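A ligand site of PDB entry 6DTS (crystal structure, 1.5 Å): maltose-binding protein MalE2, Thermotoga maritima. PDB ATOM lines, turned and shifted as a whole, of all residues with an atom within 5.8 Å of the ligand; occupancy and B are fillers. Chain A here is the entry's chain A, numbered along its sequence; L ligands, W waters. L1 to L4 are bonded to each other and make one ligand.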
ATOM      1  N   SER A  10      -2.219  18.916  25.271  1.00  0.00           N
ATOM      2  CA  SER A  10      -1.480  19.672  26.273  1.00  0.00           C
ATOM      3  C   SER A  10      -2.396  20.597  27.062  1.00  0.00           C
ATOM      4  O   SER A  10      -3.586  20.744  26.779  1.00  0.00           O
ATOM      5  CB  SER A  10      -0.368  20.507  25.613  1.00  0.00           C
ATOM      6  OG  SER A  10      -0.885  21.711  25.079  1.00  0.00           O
ATOM      7  N   GLU A  11      -1.823  21.246  28.064  1.00  0.00           N
ATOM      8  CA  GLU A  11      -2.607  22.155  28.866  1.00  0.00           C
ATOM      9  C   GLU A  11      -3.176  23.328  28.087  1.00  0.00           C
ATOM     10  O   GLU A  11      -4.159  23.936  28.542  1.00  0.00           O
ATOM     11  CB  GLU A  11      -1.816  22.696  30.052  1.00  0.00           C
ATOM     12  CG  GLU A  11      -0.738  23.709  29.702  1.00  0.00           C
ATOM     13  CD  GLU A  11       0.417  23.100  28.958  1.00  0.00           C
ATOM     14  OE1 GLU A  11       0.661  21.882  29.069  1.00  0.00           O
ATOM     15  OE2 GLU A  11       1.127  23.843  28.223  1.00  0.00           O
ATOM     16  N   LYS A  12      -2.579  23.679  26.951  1.00  0.00           N
ATOM     17  CA  LYS A  12      -3.067  24.851  26.227  1.00  0.00           C
ATOM     18  C   LYS A  12      -4.442  24.625  25.643  1.00  0.00           C
ATOM     19  O   LYS A  12      -5.201  25.593  25.489  1.00  0.00           O
ATOM     20  CB  LYS A  12      -2.109  25.229  25.095  1.00  0.00           C
ATOM     21  CG  LYS A  12      -0.692  25.585  25.576  1.00  0.00           C
ATOM     22  CD  LYS A  12      -0.704  26.834  26.420  1.00  0.00           C
ATOM     23  CE  LYS A  12       0.714  27.075  26.905  1.00  0.00           C
ATOM     24  NZ  LYS A  12       0.713  28.098  28.025  1.00  0.00           N
ATOM     25  N   GLN A  13      -4.787  23.371  25.319  1.00  0.00           N
ATOM     26  CA  GLN A  13      -6.045  23.106  24.660  1.00  0.00           C
ATOM     27  C   GLN A  13      -7.101  22.456  25.538  1.00  0.00           C
ATOM     28  O   GLN A  13      -8.221  22.332  25.067  1.00  0.00           O
ATOM     29  CB  GLN A  13      -5.850  22.222  23.423  1.00  0.00           C
ATOM     30  CG  GLN A  13      -4.821  22.785  22.428  1.00  0.00           C
ATOM     31  CD  GLN A  13      -3.431  22.185  22.653  1.00  0.00           C
ATOM     32  OE1 GLN A  13      -3.174  21.595  23.704  1.00  0.00           O
ATOM     33  NE2 GLN A  13      -2.523  22.358  21.684  1.00  0.00           N
ATOM     34  N   PHE A  39       2.908  18.007  26.974  1.00  0.00           N
ATOM     35  CA  PHE A  39       3.134  17.914  25.530  1.00  0.00           C
ATOM     36  C   PHE A  39       4.268  16.947  25.200  1.00  0.00           C
ATOM     37  O   PHE A  39       4.167  16.139  24.275  1.00  0.00           O
ATOM     38  CB  PHE A  39       3.391  19.300  24.899  1.00  0.00           C
ATOM     39  CG  PHE A  39       3.731  19.224  23.448  1.00  0.00           C
ATOM     40  CD1 PHE A  39       2.720  19.191  22.489  1.00  0.00           C
ATOM     41  CD2 PHE A  39       5.043  19.087  23.020  1.00  0.00           C
ATOM     42  CE1 PHE A  39       2.991  19.059  21.153  1.00  0.00           C
ATOM     43  CE2 PHE A  39       5.329  18.958  21.618  1.00  0.00           C
ATOM     44  CZ  PHE A  39       4.272  18.951  20.699  1.00  0.00           C
ATOM     45  N   GLY A  40       5.354  17.016  25.974  1.00  0.00           N
ATOM     46  CA  GLY A  40       6.543  16.214  25.743  1.00  0.00           C
ATOM     47  C   GLY A  40       6.345  14.735  25.979  1.00  0.00           C
ATOM     48  O   GLY A  40       7.252  13.964  25.657  1.00  0.00           O
ATOM     49  N   LYS A  43       3.409  11.961  22.350  1.00  0.00           N
ATOM     50  CA  LYS A  43       3.780  10.974  21.348  1.00  0.00           C
ATOM     51  C   LYS A  43       4.356   9.745  22.002  1.00  0.00           C
ATOM     52  O   LYS A  43       4.014   8.636  21.609  1.00  0.00           O
ATOM     53  CB  LYS A  43       4.741  11.551  20.308  1.00  0.00           C
ATOM     54  CG  LYS A  43       4.953  10.571  19.114  1.00  0.00           C
ATOM     55  CD  LYS A  43       5.948  11.098  18.114  1.00  0.00           C
ATOM     56  CE  LYS A  43       7.274  11.055  18.789  1.00  0.00           C
ATOM     57  NZ  LYS A  43       8.392  10.604  18.032  1.00  0.00           N
ATOM     58  N   SER A  44       5.254   9.912  22.985  1.00  0.00           N
ATOM     59  CA  SER A  44       5.887   8.747  23.608  1.00  0.00           C
ATOM     60  C   SER A  44       4.862   7.863  24.298  1.00  0.00           C
ATOM     61  O   SER A  44       4.940   6.631  24.215  1.00  0.00           O
ATOM     62  CB  SER A  44       7.023   9.180  24.560  1.00  0.00           C
ATOM     63  OG  SER A  44       6.583   9.984  25.628  1.00  0.00           O
ATOM     64  N   ALA A  62       1.860  17.951  17.163  1.00  0.00           N
ATOM     65  CA  ALA A  62       2.617  18.573  16.084  1.00  0.00           C
ATOM     66  C   ALA A  62       2.746  17.658  14.871  1.00  0.00           C
ATOM     67  O   ALA A  62       2.836  16.428  14.983  1.00  0.00           O
ATOM     68  CB  ALA A  62       4.010  18.952  16.561  1.00  0.00           C
ATOM     69  N   HIS A  63       2.829  18.289  13.683  1.00  0.00           N
ATOM     70  CA  HIS A  63       2.771  17.530  12.441  1.00  0.00           C
ATOM     71  C   HIS A  63       4.014  16.670  12.214  1.00  0.00           C
ATOM     72  O   HIS A  63       3.951  15.747  11.386  1.00  0.00           O
ATOM     73  CB  HIS A  63       2.610  18.483  11.247  1.00  0.00           C
ATOM     74  CG  HIS A  63       3.874  19.183  10.844  1.00  0.00           C
ATOM     75  ND1 HIS A  63       4.237  20.423  11.366  1.00  0.00           N
ATOM     76  CD2 HIS A  63       4.805  18.840   9.925  1.00  0.00           C
ATOM     77  CE1 HIS A  63       5.393  20.777  10.805  1.00  0.00           C
ATOM     78  NE2 HIS A  63       5.759  19.828   9.954  1.00  0.00           N
ATOM     79  N   ASP A  64       5.133  16.935  12.885  1.00  0.00           N
ATOM     80  CA  ASP A  64       6.327  16.138  12.587  1.00  0.00           C
ATOM     81  C   ASP A  64       6.147  14.701  12.995  1.00  0.00           C
ATOM     82  O   ASP A  64       6.881  13.840  12.481  1.00  0.00           O
ATOM     83  CB  ASP A  64       7.578  16.732  13.224  1.00  0.00           C
ATOM     84  CG  ASP A  64       7.485  16.880  14.745  1.00  0.00           C
ATOM     85  OD1 ASP A  64       6.670  17.687  15.230  1.00  0.00           O
ATOM     86  OD2 ASP A  64       8.263  16.180  15.441  1.00  0.00           O
ATOM     87  N   TRP A  65       5.164  14.423  13.859  1.00  0.00           N
ATOM     88  CA  TRP A  65       4.921  13.051  14.312  1.00  0.00           C
ATOM     89  C   TRP A  65       4.325  12.178  13.208  1.00  0.00           C
ATOM     90  O   TRP A  65       4.319  10.949  13.331  1.00  0.00           O
ATOM     91  CB  TRP A  65       3.922  13.063  15.460  1.00  0.00           C
ATOM     92  CG  TRP A  65       4.232  13.918  16.621  1.00  0.00           C
ATOM     93  CD1 TRP A  65       5.393  14.569  16.900  1.00  0.00           C
ATOM     94  CD2 TRP A  65       3.319  14.212  17.695  1.00  0.00           C
ATOM     95  NE1 TRP A  65       5.257  15.259  18.098  1.00  0.00           N
ATOM     96  CE2 TRP A  65       3.996  15.049  18.609  1.00  0.00           C
ATOM     97  CE3 TRP A  65       2.019  13.807  17.976  1.00  0.00           C
ATOM     98  CZ2 TRP A  65       3.408  15.520  19.800  1.00  0.00           C
ATOM     99  CZ3 TRP A  65       1.387  14.299  19.120  1.00  0.00           C
ATOM    100  CH2 TRP A  65       2.095  15.162  20.033  1.00  0.00           C
ATOM    101  N   GLU A 109       2.633  27.726  13.376  1.00  0.00           N
ATOM    102  CA  GLU A 109       3.433  28.416  14.391  1.00  0.00           C
ATOM    103  C   GLU A 109       4.920  28.392  14.062  1.00  0.00           C
ATOM    104  O   GLU A 109       5.439  27.480  13.415  1.00  0.00           O
ATOM    105  CB  GLU A 109       3.180  27.843  15.782  1.00  0.00           C
ATOM    106  CG  GLU A 109       3.596  26.361  15.867  1.00  0.00           C
ATOM    107  CD  GLU A 109       3.138  25.646  17.123  1.00  0.00           C
ATOM    108  OE1 GLU A 109       2.268  26.160  17.850  1.00  0.00           O
ATOM    109  OE2 GLU A 109       3.656  24.549  17.329  1.00  0.00           O
ATOM    110  N   ASP A 151      15.450  27.744  25.854  1.00  0.00           N
ATOM    111  CA  ASP A 151      15.694  26.290  25.946  1.00  0.00           C
ATOM    112  C   ASP A 151      16.784  25.850  24.963  1.00  0.00           C
ATOM    113  O   ASP A 151      16.500  25.173  23.972  1.00  0.00           O
ATOM    114  CB  ASP A 151      14.376  25.560  25.676  1.00  0.00           C
ATOM    115  CG  ASP A 151      14.396  24.085  26.078  1.00  0.00           C
ATOM    116  OD1 ASP A 151      15.336  23.595  26.771  1.00  0.00           O
ATOM    117  OD2 ASP A 151      13.412  23.441  25.719  1.00  0.00           O
ATOM    118  N   ASN A 154      17.632  22.289  23.353  1.00  0.00           N
ATOM    119  CA  ASN A 154      16.526  21.676  22.636  1.00  0.00           C
ATOM    120  C   ASN A 154      16.642  22.065  21.160  1.00  0.00           C
ATOM    121  O   ASN A 154      16.590  23.254  20.809  1.00  0.00           O
ATOM    122  CB  ASN A 154      15.229  22.227  23.238  1.00  0.00           C
ATOM    123  CG  ASN A 154      13.950  21.594  22.655  1.00  0.00           C
ATOM    124  OD1 ASN A 154      13.980  21.062  21.534  1.00  0.00           O
ATOM    125  ND2 ASN A 154      12.844  21.639  23.415  1.00  0.00           N
ATOM    126  N   PHE A 155      16.834  21.075  20.288  1.00  0.00           N
ATOM    127  CA  PHE A 155      17.054  21.409  18.879  1.00  0.00           C
ATOM    128  C   PHE A 155      15.900  22.197  18.256  1.00  0.00           C
ATOM    129  O   PHE A 155      16.125  23.016  17.333  1.00  0.00           O
ATOM    130  CB  PHE A 155      17.335  20.143  18.058  1.00  0.00           C
ATOM    131  CG  PHE A 155      17.544  20.376  16.563  1.00  0.00           C
ATOM    132  CD1 PHE A 155      18.477  21.327  16.079  1.00  0.00           C
ATOM    133  CD2 PHE A 155      16.819  19.639  15.636  1.00  0.00           C
ATOM    134  CE1 PHE A 155      18.616  21.530  14.702  1.00  0.00           C
ATOM    135  CE2 PHE A 155      16.965  19.831  14.254  1.00  0.00           C
ATOM    136  CZ  PHE A 155      17.853  20.777  13.780  1.00  0.00           C
ATOM    137  N   TYR A 156      14.668  21.972  18.718  1.00  0.00           N
ATOM    138  CA  TYR A 156      13.554  22.739  18.201  1.00  0.00           C
ATOM    139  C   TYR A 156      13.778  24.252  18.347  1.00  0.00           C
ATOM    140  O   TYR A 156      13.550  25.022  17.385  1.00  0.00           O
ATOM    141  CB  TYR A 156      12.244  22.298  18.873  1.00  0.00           C
ATOM    142  CG  TYR A 156      11.078  23.103  18.399  1.00  0.00           C
ATOM    143  CD1 TYR A 156      10.436  22.768  17.242  1.00  0.00           C
ATOM    144  CD2 TYR A 156      10.678  24.230  19.096  1.00  0.00           C
ATOM    145  CE1 TYR A 156       9.370  23.518  16.726  1.00  0.00           C
ATOM    146  CE2 TYR A 156       9.611  25.013  18.624  1.00  0.00           C
ATOM    147  CZ  TYR A 156       8.925  24.644  17.447  1.00  0.00           C
ATOM    148  OH  TYR A 156       7.885  25.447  17.005  1.00  0.00           O
ATOM    149  N   PHE A 157      14.288  24.691  19.508  1.00  0.00           N
ATOM    150  CA  PHE A 157      14.476  26.119  19.762  1.00  0.00           C
ATOM    151  C   PHE A 157      15.802  26.652  19.242  1.00  0.00           C
ATOM    152  O   PHE A 157      15.900  27.853  18.984  1.00  0.00           O
ATOM    153  CB  PHE A 157      14.316  26.429  21.242  1.00  0.00           C
ATOM    154  CG  PHE A 157      12.932  26.204  21.760  1.00  0.00           C
ATOM    155  CD1 PHE A 157      11.920  27.078  21.498  1.00  0.00           C
ATOM    156  CD2 PHE A 157      12.665  25.076  22.551  1.00  0.00           C
ATOM    157  CE1 PHE A 157      10.603  26.861  21.990  1.00  0.00           C
ATOM    158  CE2 PHE A 157      11.339  24.861  23.043  1.00  0.00           C
ATOM    159  CZ  PHE A 157      10.344  25.753  22.783  1.00  0.00           C
ATOM    160  N   TYR A 211      13.366  25.085  29.195  1.00  0.00           N
ATOM    161  CA  TYR A 211      12.079  25.728  28.928  1.00  0.00           C
ATOM    162  C   TYR A 211      11.455  26.256  30.202  1.00  0.00           C
ATOM    163  O   TYR A 211      10.995  27.399  30.252  1.00  0.00           O
ATOM    164  CB  TYR A 211      11.116  24.773  28.203  1.00  0.00           C
ATOM    165  CG  TYR A 211       9.871  25.474  27.719  1.00  0.00           C
ATOM    166  CD1 TYR A 211       9.808  26.101  26.443  1.00  0.00           C
ATOM    167  CD2 TYR A 211       8.741  25.550  28.538  1.00  0.00           C
ATOM    168  CE1 TYR A 211       8.685  26.737  26.013  1.00  0.00           C
ATOM    169  CE2 TYR A 211       7.602  26.228  28.128  1.00  0.00           C
ATOM    170  CZ  TYR A 211       7.563  26.804  26.841  1.00  0.00           C
ATOM    171  OH  TYR A 211       6.436  27.457  26.407  1.00  0.00           O
ATOM    172  N   ASN A 228      10.417  31.960  22.132  1.00  0.00           N
ATOM    173  CA  ASN A 228       9.273  31.112  22.455  1.00  0.00           C
ATOM    174  C   ASN A 228       8.188  31.331  21.399  1.00  0.00           C
ATOM    175  O   ASN A 228       8.287  32.224  20.557  1.00  0.00           O
ATOM    176  CB  ASN A 228       8.769  31.345  23.884  1.00  0.00           C
ATOM    177  CG  ASN A 228       8.080  30.083  24.451  1.00  0.00           C
ATOM    178  OD1 ASN A 228       7.983  29.052  23.764  1.00  0.00           O
ATOM    179  ND2 ASN A 228       7.612  30.160  25.704  1.00  0.00           N
ATOM    180  N   TRP A 231       1.979  30.095  21.568  1.00  0.00           N
ATOM    181  CA  TRP A 231       1.301  29.302  22.603  1.00  0.00           C
ATOM    182  C   TRP A 231       1.499  29.851  23.996  1.00  0.00           C
ATOM    183  O   TRP A 231       0.620  29.627  24.859  1.00  0.00           O
ATOM    184  CB  TRP A 231       1.722  27.818  22.558  1.00  0.00           C
ATOM    185  CG  TRP A 231       3.220  27.628  22.752  1.00  0.00           C
ATOM    186  CD1 TRP A 231       3.923  27.607  23.943  1.00  0.00           C
ATOM    187  CD2 TRP A 231       4.164  27.426  21.728  1.00  0.00           C
ATOM    188  NE1 TRP A 231       5.262  27.450  23.701  1.00  0.00           N
ATOM    189  CE2 TRP A 231       5.447  27.314  22.340  1.00  0.00           C
ATOM    190  CE3 TRP A 231       4.066  27.298  20.346  1.00  0.00           C
ATOM    191  CZ2 TRP A 231       6.631  27.102  21.586  1.00  0.00           C
ATOM    192  CZ3 TRP A 231       5.214  27.079  19.602  1.00  0.00           C
ATOM    193  CH2 TRP A 231       6.489  27.003  20.221  1.00  0.00           C
ATOM    194  N   GLY A 262       5.860  24.843  12.613  1.00  0.00           N
ATOM    195  CA  GLY A 262       5.114  23.705  13.096  1.00  0.00           C
ATOM    196  C   GLY A 262       3.637  23.907  12.783  1.00  0.00           C
ATOM    197  O   GLY A 262       3.136  25.045  12.748  1.00  0.00           O
ATOM    198  N   GLN A 264      -0.055  22.472  14.274  1.00  0.00           N
ATOM    199  CA  GLN A 264      -0.718  21.692  15.319  1.00  0.00           C
ATOM    200  C   GLN A 264      -2.055  21.199  14.779  1.00  0.00           C
ATOM    201  O   GLN A 264      -2.748  21.920  14.047  1.00  0.00           O
ATOM    202  CB  GLN A 264      -0.986  22.553  16.571  1.00  0.00           C
ATOM    203  CG  GLN A 264       0.246  23.069  17.240  1.00  0.00           C
ATOM    204  CD  GLN A 264       0.986  22.017  18.052  1.00  0.00           C
ATOM    205  OE1 GLN A 264       0.356  21.122  18.636  1.00  0.00           O
ATOM    206  NE2 GLN A 264       2.275  22.144  18.117  1.00  0.00           N
ATOM    207  N   ASP A 299      -6.812  29.538  22.319  1.00  0.00           N
ATOM    208  CA  ASP A 299      -5.426  29.164  22.116  1.00  0.00           C
ATOM    209  C   ASP A 299      -5.001  29.902  20.842  1.00  0.00           C
ATOM    210  O   ASP A 299      -5.061  29.362  19.740  1.00  0.00           O
ATOM    211  CB  ASP A 299      -5.293  27.639  21.996  1.00  0.00           C
ATOM    212  CG  ASP A 299      -3.854  27.152  21.824  1.00  0.00           C
ATOM    213  OD1 ASP A 299      -2.925  27.987  21.888  1.00  0.00           O
ATOM    214  OD2 ASP A 299      -3.684  25.948  21.580  1.00  0.00           O
ATOM    215  N   ARG A 301      -3.060  30.778  18.499  1.00  0.00           N
ATOM    216  CA  ARG A 301      -2.069  30.556  17.464  1.00  0.00           C
ATOM    217  C   ARG A 301      -2.666  30.874  16.094  1.00  0.00           C
ATOM    218  O   ARG A 301      -3.881  30.879  15.924  1.00  0.00           O
ATOM    219  CB  ARG A 301      -1.647  29.086  17.510  1.00  0.00           C
ATOM    220  CG  ARG A 301      -1.199  28.656  18.918  1.00  0.00           C
ATOM    221  CD  ARG A 301      -0.730  27.254  18.933  1.00  0.00           C
ATOM    222  NE  ARG A 301      -0.950  26.672  20.245  1.00  0.00           N
ATOM    223  CZ  ARG A 301      -0.264  25.639  20.757  1.00  0.00           C
ATOM    224  NH1 ARG A 301       0.800  25.086  20.141  1.00  0.00           N
ATOM    225  NH2 ARG A 301      -0.632  25.188  21.929  1.00  0.00           N
ATOM    226  N   MET A 331       8.846  21.726   9.728  1.00  0.00           N
ATOM    227  CA  MET A 331       9.583  20.561  10.189  1.00  0.00           C
ATOM    228  C   MET A 331       9.348  19.409   9.229  1.00  0.00           C
ATOM    229  O   MET A 331       8.223  19.268   8.712  1.00  0.00           O
ATOM    230  CB  MET A 331       9.125  20.127  11.585  1.00  0.00           C
ATOM    231  CG  MET A 331       9.351  21.156  12.695  1.00  0.00           C
ATOM    232  SD  MET A 331       8.872  20.519  14.311  1.00  0.00           S
ATOM    233  CE  MET A 331       7.105  20.753  14.298  1.00  0.00           C
ATOM    234  N   ALA A 338      12.226  11.043  13.540  1.00  0.00           N
ATOM    235  CA  ALA A 338      12.145  10.622  14.935  1.00  0.00           C
ATOM    236  C   ALA A 338      13.471  10.704  15.683  1.00  0.00           C
ATOM    237  O   ALA A 338      13.483  11.235  16.804  1.00  0.00           O
ATOM    238  CB  ALA A 338      11.566   9.187  15.015  1.00  0.00           C
ATOM    239  N   TRP A 341      15.733  14.582  16.826  1.00  0.00           N
ATOM    240  CA  TRP A 341      15.611  15.452  17.992  1.00  0.00           C
ATOM    241  C   TRP A 341      16.584  15.077  19.093  1.00  0.00           C
ATOM    242  O   TRP A 341      17.225  15.949  19.674  1.00  0.00           O
ATOM    243  CB  TRP A 341      14.189  15.362  18.531  1.00  0.00           C
ATOM    244  CG  TRP A 341      13.141  15.776  17.539  1.00  0.00           C
ATOM    245  CD1 TRP A 341      12.199  14.958  16.972  1.00  0.00           C
ATOM    246  CD2 TRP A 341      12.911  17.097  17.005  1.00  0.00           C
ATOM    247  NE1 TRP A 341      11.384  15.709  16.106  1.00  0.00           N
ATOM    248  CE2 TRP A 341      11.812  17.006  16.121  1.00  0.00           C
ATOM    249  CE3 TRP A 341      13.537  18.343  17.184  1.00  0.00           C
ATOM    250  CZ2 TRP A 341      11.325  18.122  15.424  1.00  0.00           C
ATOM    251  CZ3 TRP A 341      13.049  19.430  16.493  1.00  0.00           C
ATOM    252  CH2 TRP A 341      11.988  19.325  15.610  1.00  0.00           C
ATOM    253  N   SER A 342      16.659  13.776  19.433  1.00  0.00           N
ATOM    254  CA  SER A 342      17.527  13.348  20.536  1.00  0.00           C
ATOM    255  C   SER A 342      18.996  13.474  20.160  1.00  0.00           C
ATOM    256  O   SER A 342      19.809  13.883  20.990  1.00  0.00           O
ATOM    257  CB  SER A 342      17.238  11.903  20.934  1.00  0.00           C
ATOM    258  OG  SER A 342      18.156  11.480  21.911  1.00  0.00           O
HETATM  259  C1  LIG L   1       2.637  23.644  25.164  1.00  0.00           C
HETATM  260  C2  LIG L   1       2.218  23.713  23.742  1.00  0.00           C
HETATM  261  C3  LIG L   1       3.121  23.003  22.826  1.00  0.00           C
HETATM  262  C4  LIG L   1       4.521  23.499  22.957  1.00  0.00           C
HETATM  263  C5  LIG L   1       5.002  23.196  24.401  1.00  0.00           C
HETATM  264  C6  LIG L   1       6.304  23.741  24.713  1.00  0.00           C
HETATM  265  O1  LIG L   1       2.419  22.333  25.552  1.00  0.00           O
HETATM  266  O2  LIG L   1       0.833  23.226  23.608  1.00  0.00           O
HETATM  267  O3  LIG L   1       2.646  23.247  21.468  1.00  0.00           O
HETATM  268  O4  LIG L   1       5.368  22.757  22.079  1.00  0.00           O
HETATM  269  O5  LIG L   1       4.065  23.934  25.348  1.00  0.00           O
HETATM  270  O6  LIG L   1       6.815  23.260  25.977  1.00  0.00           O
HETATM  271  C1  LG2 L   2       6.232  23.535  21.274  1.00  0.00           C
HETATM  272  C2  LG2 L   2       5.981  23.246  19.854  1.00  0.00           C
HETATM  273  C3  LG2 L   2       6.381  21.844  19.530  1.00  0.00           C
HETATM  274  C4  LG2 L   2       7.809  21.515  19.910  1.00  0.00           C
HETATM  275  C5  LG2 L   2       8.107  21.826  21.404  1.00  0.00           C
HETATM  276  C6  LG2 L   2       9.496  21.760  21.726  1.00  0.00           C
HETATM  277  O1  LG2 L   2       4.546  23.395  19.579  1.00  0.00           O
HETATM  278  O2  LG2 L   2       6.203  21.550  18.101  1.00  0.00           O
HETATM  279  O3  LG2 L   2       8.117  20.107  19.678  1.00  0.00           O
HETATM  280  O4  LG2 L   2       7.626  23.226  21.622  1.00  0.00           O
HETATM  281  O5  LG2 L   2       9.728  21.582  23.107  1.00  0.00           O
HETATM  282  C1  LG3 L   3       8.964  19.833  18.587  1.00  0.00           C
HETATM  283  C2  LG3 L   3       8.458  18.618  17.912  1.00  0.00           C
HETATM  284  C3  LG3 L   3       8.474  17.400  18.807  1.00  0.00           C
HETATM  285  C4  LG3 L   3       9.849  17.153  19.352  1.00  0.00           C
HETATM  286  C5  LG3 L   3      10.349  18.367  20.144  1.00  0.00           C
HETATM  287  C6  LG3 L   3      11.717  18.262  20.592  1.00  0.00           C
HETATM  288  O1  LG3 L   3       7.087  18.922  17.485  1.00  0.00           O
HETATM  289  O2  LG3 L   3       8.003  16.241  18.031  1.00  0.00           O
HETATM  290  O3  LG3 L   3       9.808  16.082  20.318  1.00  0.00           O
HETATM  291  O4  LG3 L   3      10.276  19.532  19.168  1.00  0.00           O
HETATM  292  O5  LG3 L   3      11.962  19.295  21.556  1.00  0.00           O
HETATM  293  C1  LG4 L   4      10.331  14.853  19.843  1.00  0.00           C
HETATM  294  C2  LG4 L   4       9.483  13.716  20.264  1.00  0.00           C
HETATM  295  C3  LG4 L   4       9.459  13.491  21.729  1.00  0.00           C
HETATM  296  C4  LG4 L   4      10.877  13.324  22.225  1.00  0.00           C
HETATM  297  C5  LG4 L   4      11.706  14.569  21.933  1.00  0.00           C
HETATM  298  C6  LG4 L   4      13.063  14.428  22.346  1.00  0.00           C
HETATM  299  O1  LG4 L   4       8.146  13.956  19.748  1.00  0.00           O
HETATM  300  O2  LG4 L   4       8.711  12.221  21.944  1.00  0.00           O
HETATM  301  O3  LG4 L   4      10.871  13.228  23.639  1.00  0.00           O
HETATM  302  O4  LG4 L   4      11.698  14.730  20.411  1.00  0.00           O
HETATM  303  O5  LG4 L   4      13.658  13.340  21.663  1.00  0.00           O
HETATM  304  O   HOH W   1       6.663  15.756  21.020  1.00  0.00           O
HETATM  305  O   HOH W   2       8.270   9.977  21.207  1.00  0.00           O
HETATM  306  O   HOH W   3       8.300  16.973  22.809  1.00  0.00           O
HETATM  307  O   HOH W   4       6.915  20.357  25.862  1.00  0.00           O
HETATM  308  O   HOH W   5       9.567  15.116  24.747  1.00  0.00           O
HETATM  309  O   HOH W   6       8.703  19.314  24.186  1.00  0.00           O
HETATM  310  O   HOH W   7       9.494  22.975  25.485  1.00  0.00           O
HETATM  311  O   HOH W   8       6.032  23.742  16.276  1.00  0.00           O
HETATM  312  O   HOH W   9       5.481  23.246  28.411  1.00  0.00           O
HETATM  313  O   HOH W  10      12.616  17.982  23.973  1.00  0.00           O
HETATM  314  O   HOH W  11      14.671  11.972  18.991  1.00  0.00           O
HETATM  315  O   HOH W  12       6.715  12.381  23.477  1.00  0.00           O
HETATM  316  O   HOH W  13       0.137  21.197  21.353  1.00  0.00           O
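An oxygen (O1) of LG2 L2 sits at hydrogen-bond distance from the side-chain carboxylate (OE2) of Glu 109 (2.7 Å). The guanidinium group (NH1) of Arg 301 lies within hydrogen-bond range of an oxygen (O3) of LIG L1 (2.9 Å). An oxygen (O2) of LG3 L3 is in hydrogen-bond range of the indole nitrogen of Trp 65, at 2.9 Å. The side-chain amide nitrogen (NE2) of Gln 264 sits at hydrogen-bond distance from an oxygen (O1) of LG2 L2 (3.0 Å). OD1 of Asp 64 is in hydrogen-bond range of O1 of LG3 L3 (2.6 Å). The side-chain hydroxyl (OG) of Ser 10 is in hydrogen-bond range of an oxygen (O2) of LIG L1, at 2.7 Å. OE2 of Glu 11 sits at hydrogen-bond distance from O1 of LIG L1 (3.3 Å). The side-chain amide oxygen of Asn 154 lies within hydrogen-bond range of an oxygen (O5) of LG3 L3, 2.7 Å away.
The side-chain amide oxygen (OE1) of Gln 13 sits at hydrogen-bond distance from the side-chain hydroxyl (OG) of Ser 10, at 2.7 Å. The backbone carbonyl oxygen (O) of Met 331 lies within hydrogen-bond range of a ring nitrogen (NE2) of His 63, 2.8 Å away. The backbone NH (N) of Gly 262 is in hydrogen-bond range of the backbone carbonyl oxygen (O) of Glu 109, 2.8 Å away. NE2 of Gln 264 is in hydrogen-bond range of OE2 of Glu 109 (2.9 Å). The guanidinium group (NH1) of Arg 301 lies within salt-bridge range of the side-chain carboxylate (OE1) of Glu 109 (2.9 Å). N of Lys 12 lies close to OG of Ser 10. N of Tyr 156 lies within hydrogen-bond range of OD1 of Asn 154, 3.0 Å away. The side-chain hydroxyl of Tyr 211 is in hydrogen-bond range of the side-chain amide nitrogen of Asn 228.
Lys 12 touches the ligand. Gln 13 touches the ligand. CB of Phe 39 touches O1 of LIG L1, at 3.3 Å. Lys 43 touches the ligand. Ala 62 touches the ligand. Tyr 156 touches the ligand. Phe 157 touches the ligand. Tyr 211 touches the ligand. CZ2 of Trp 231 touches C1 of LG2 L2, at 3.6 Å. CE of Met 331 touches O1 of LG3 L3, at 3.7 Å. CB of Trp 341 touches O4 of LG4 L4, 3.2 Å away. Ser 342 touches the ligand. Hydrophobic or aromatic side chains that line the ligand: Phe 39, Ala 62, Trp 65, Tyr 156, Phe 157, Tyr 211, Trp 231, Met 331 and Trp 341. 20 residues have an atom within 4 Å of the ligand: Ser 10, Glu 11, Lys 12, Gln 13, Phe 39, Lys 43, Ala 62, Asp 64, Trp 65, Glu 109, Asn 154, Tyr 156, Phe 157, Tyr 211, Trp 231, Gln 264, Arg 301, Met 331, Trp 341 and Ser 342. The nearest printed residue that does not touch the ligand is Gly 40 (4.2 Å).
Water W2 lies within hydrogen-bond range of O2 of LG4 L4 (2.4 Å) and NZ of Lys 43 (3.2 Å). Water W12 lies within hydrogen-bond range of O2 of LG4 L4, O of Gly 40 and N of Ser 44. Water W5 lies within hydrogen-bond range of an oxygen (O3) of LG4 L4 and the backbone carbonyl oxygen (O) of Gly 40. Water W1 bridges an oxygen (O1) of LG4 L4 (2.7 Å) and the indole nitrogen (NE1) of Trp 65 (3.3 Å). Water W8 lies within hydrogen-bond range of OH of Tyr 156 (2.6 Å), OE2 of Glu 109 (2.7 Å) and O2 of LG2 L2 (2.9 Å). Water W13 lies within hydrogen-bond range of the side-chain amide oxygen of Gln 264 (2.7 Å), the side-chain amide nitrogen of Gln 13 (2.9 Å) and an oxygen (O2) of LIG L1 (3.1 Å).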
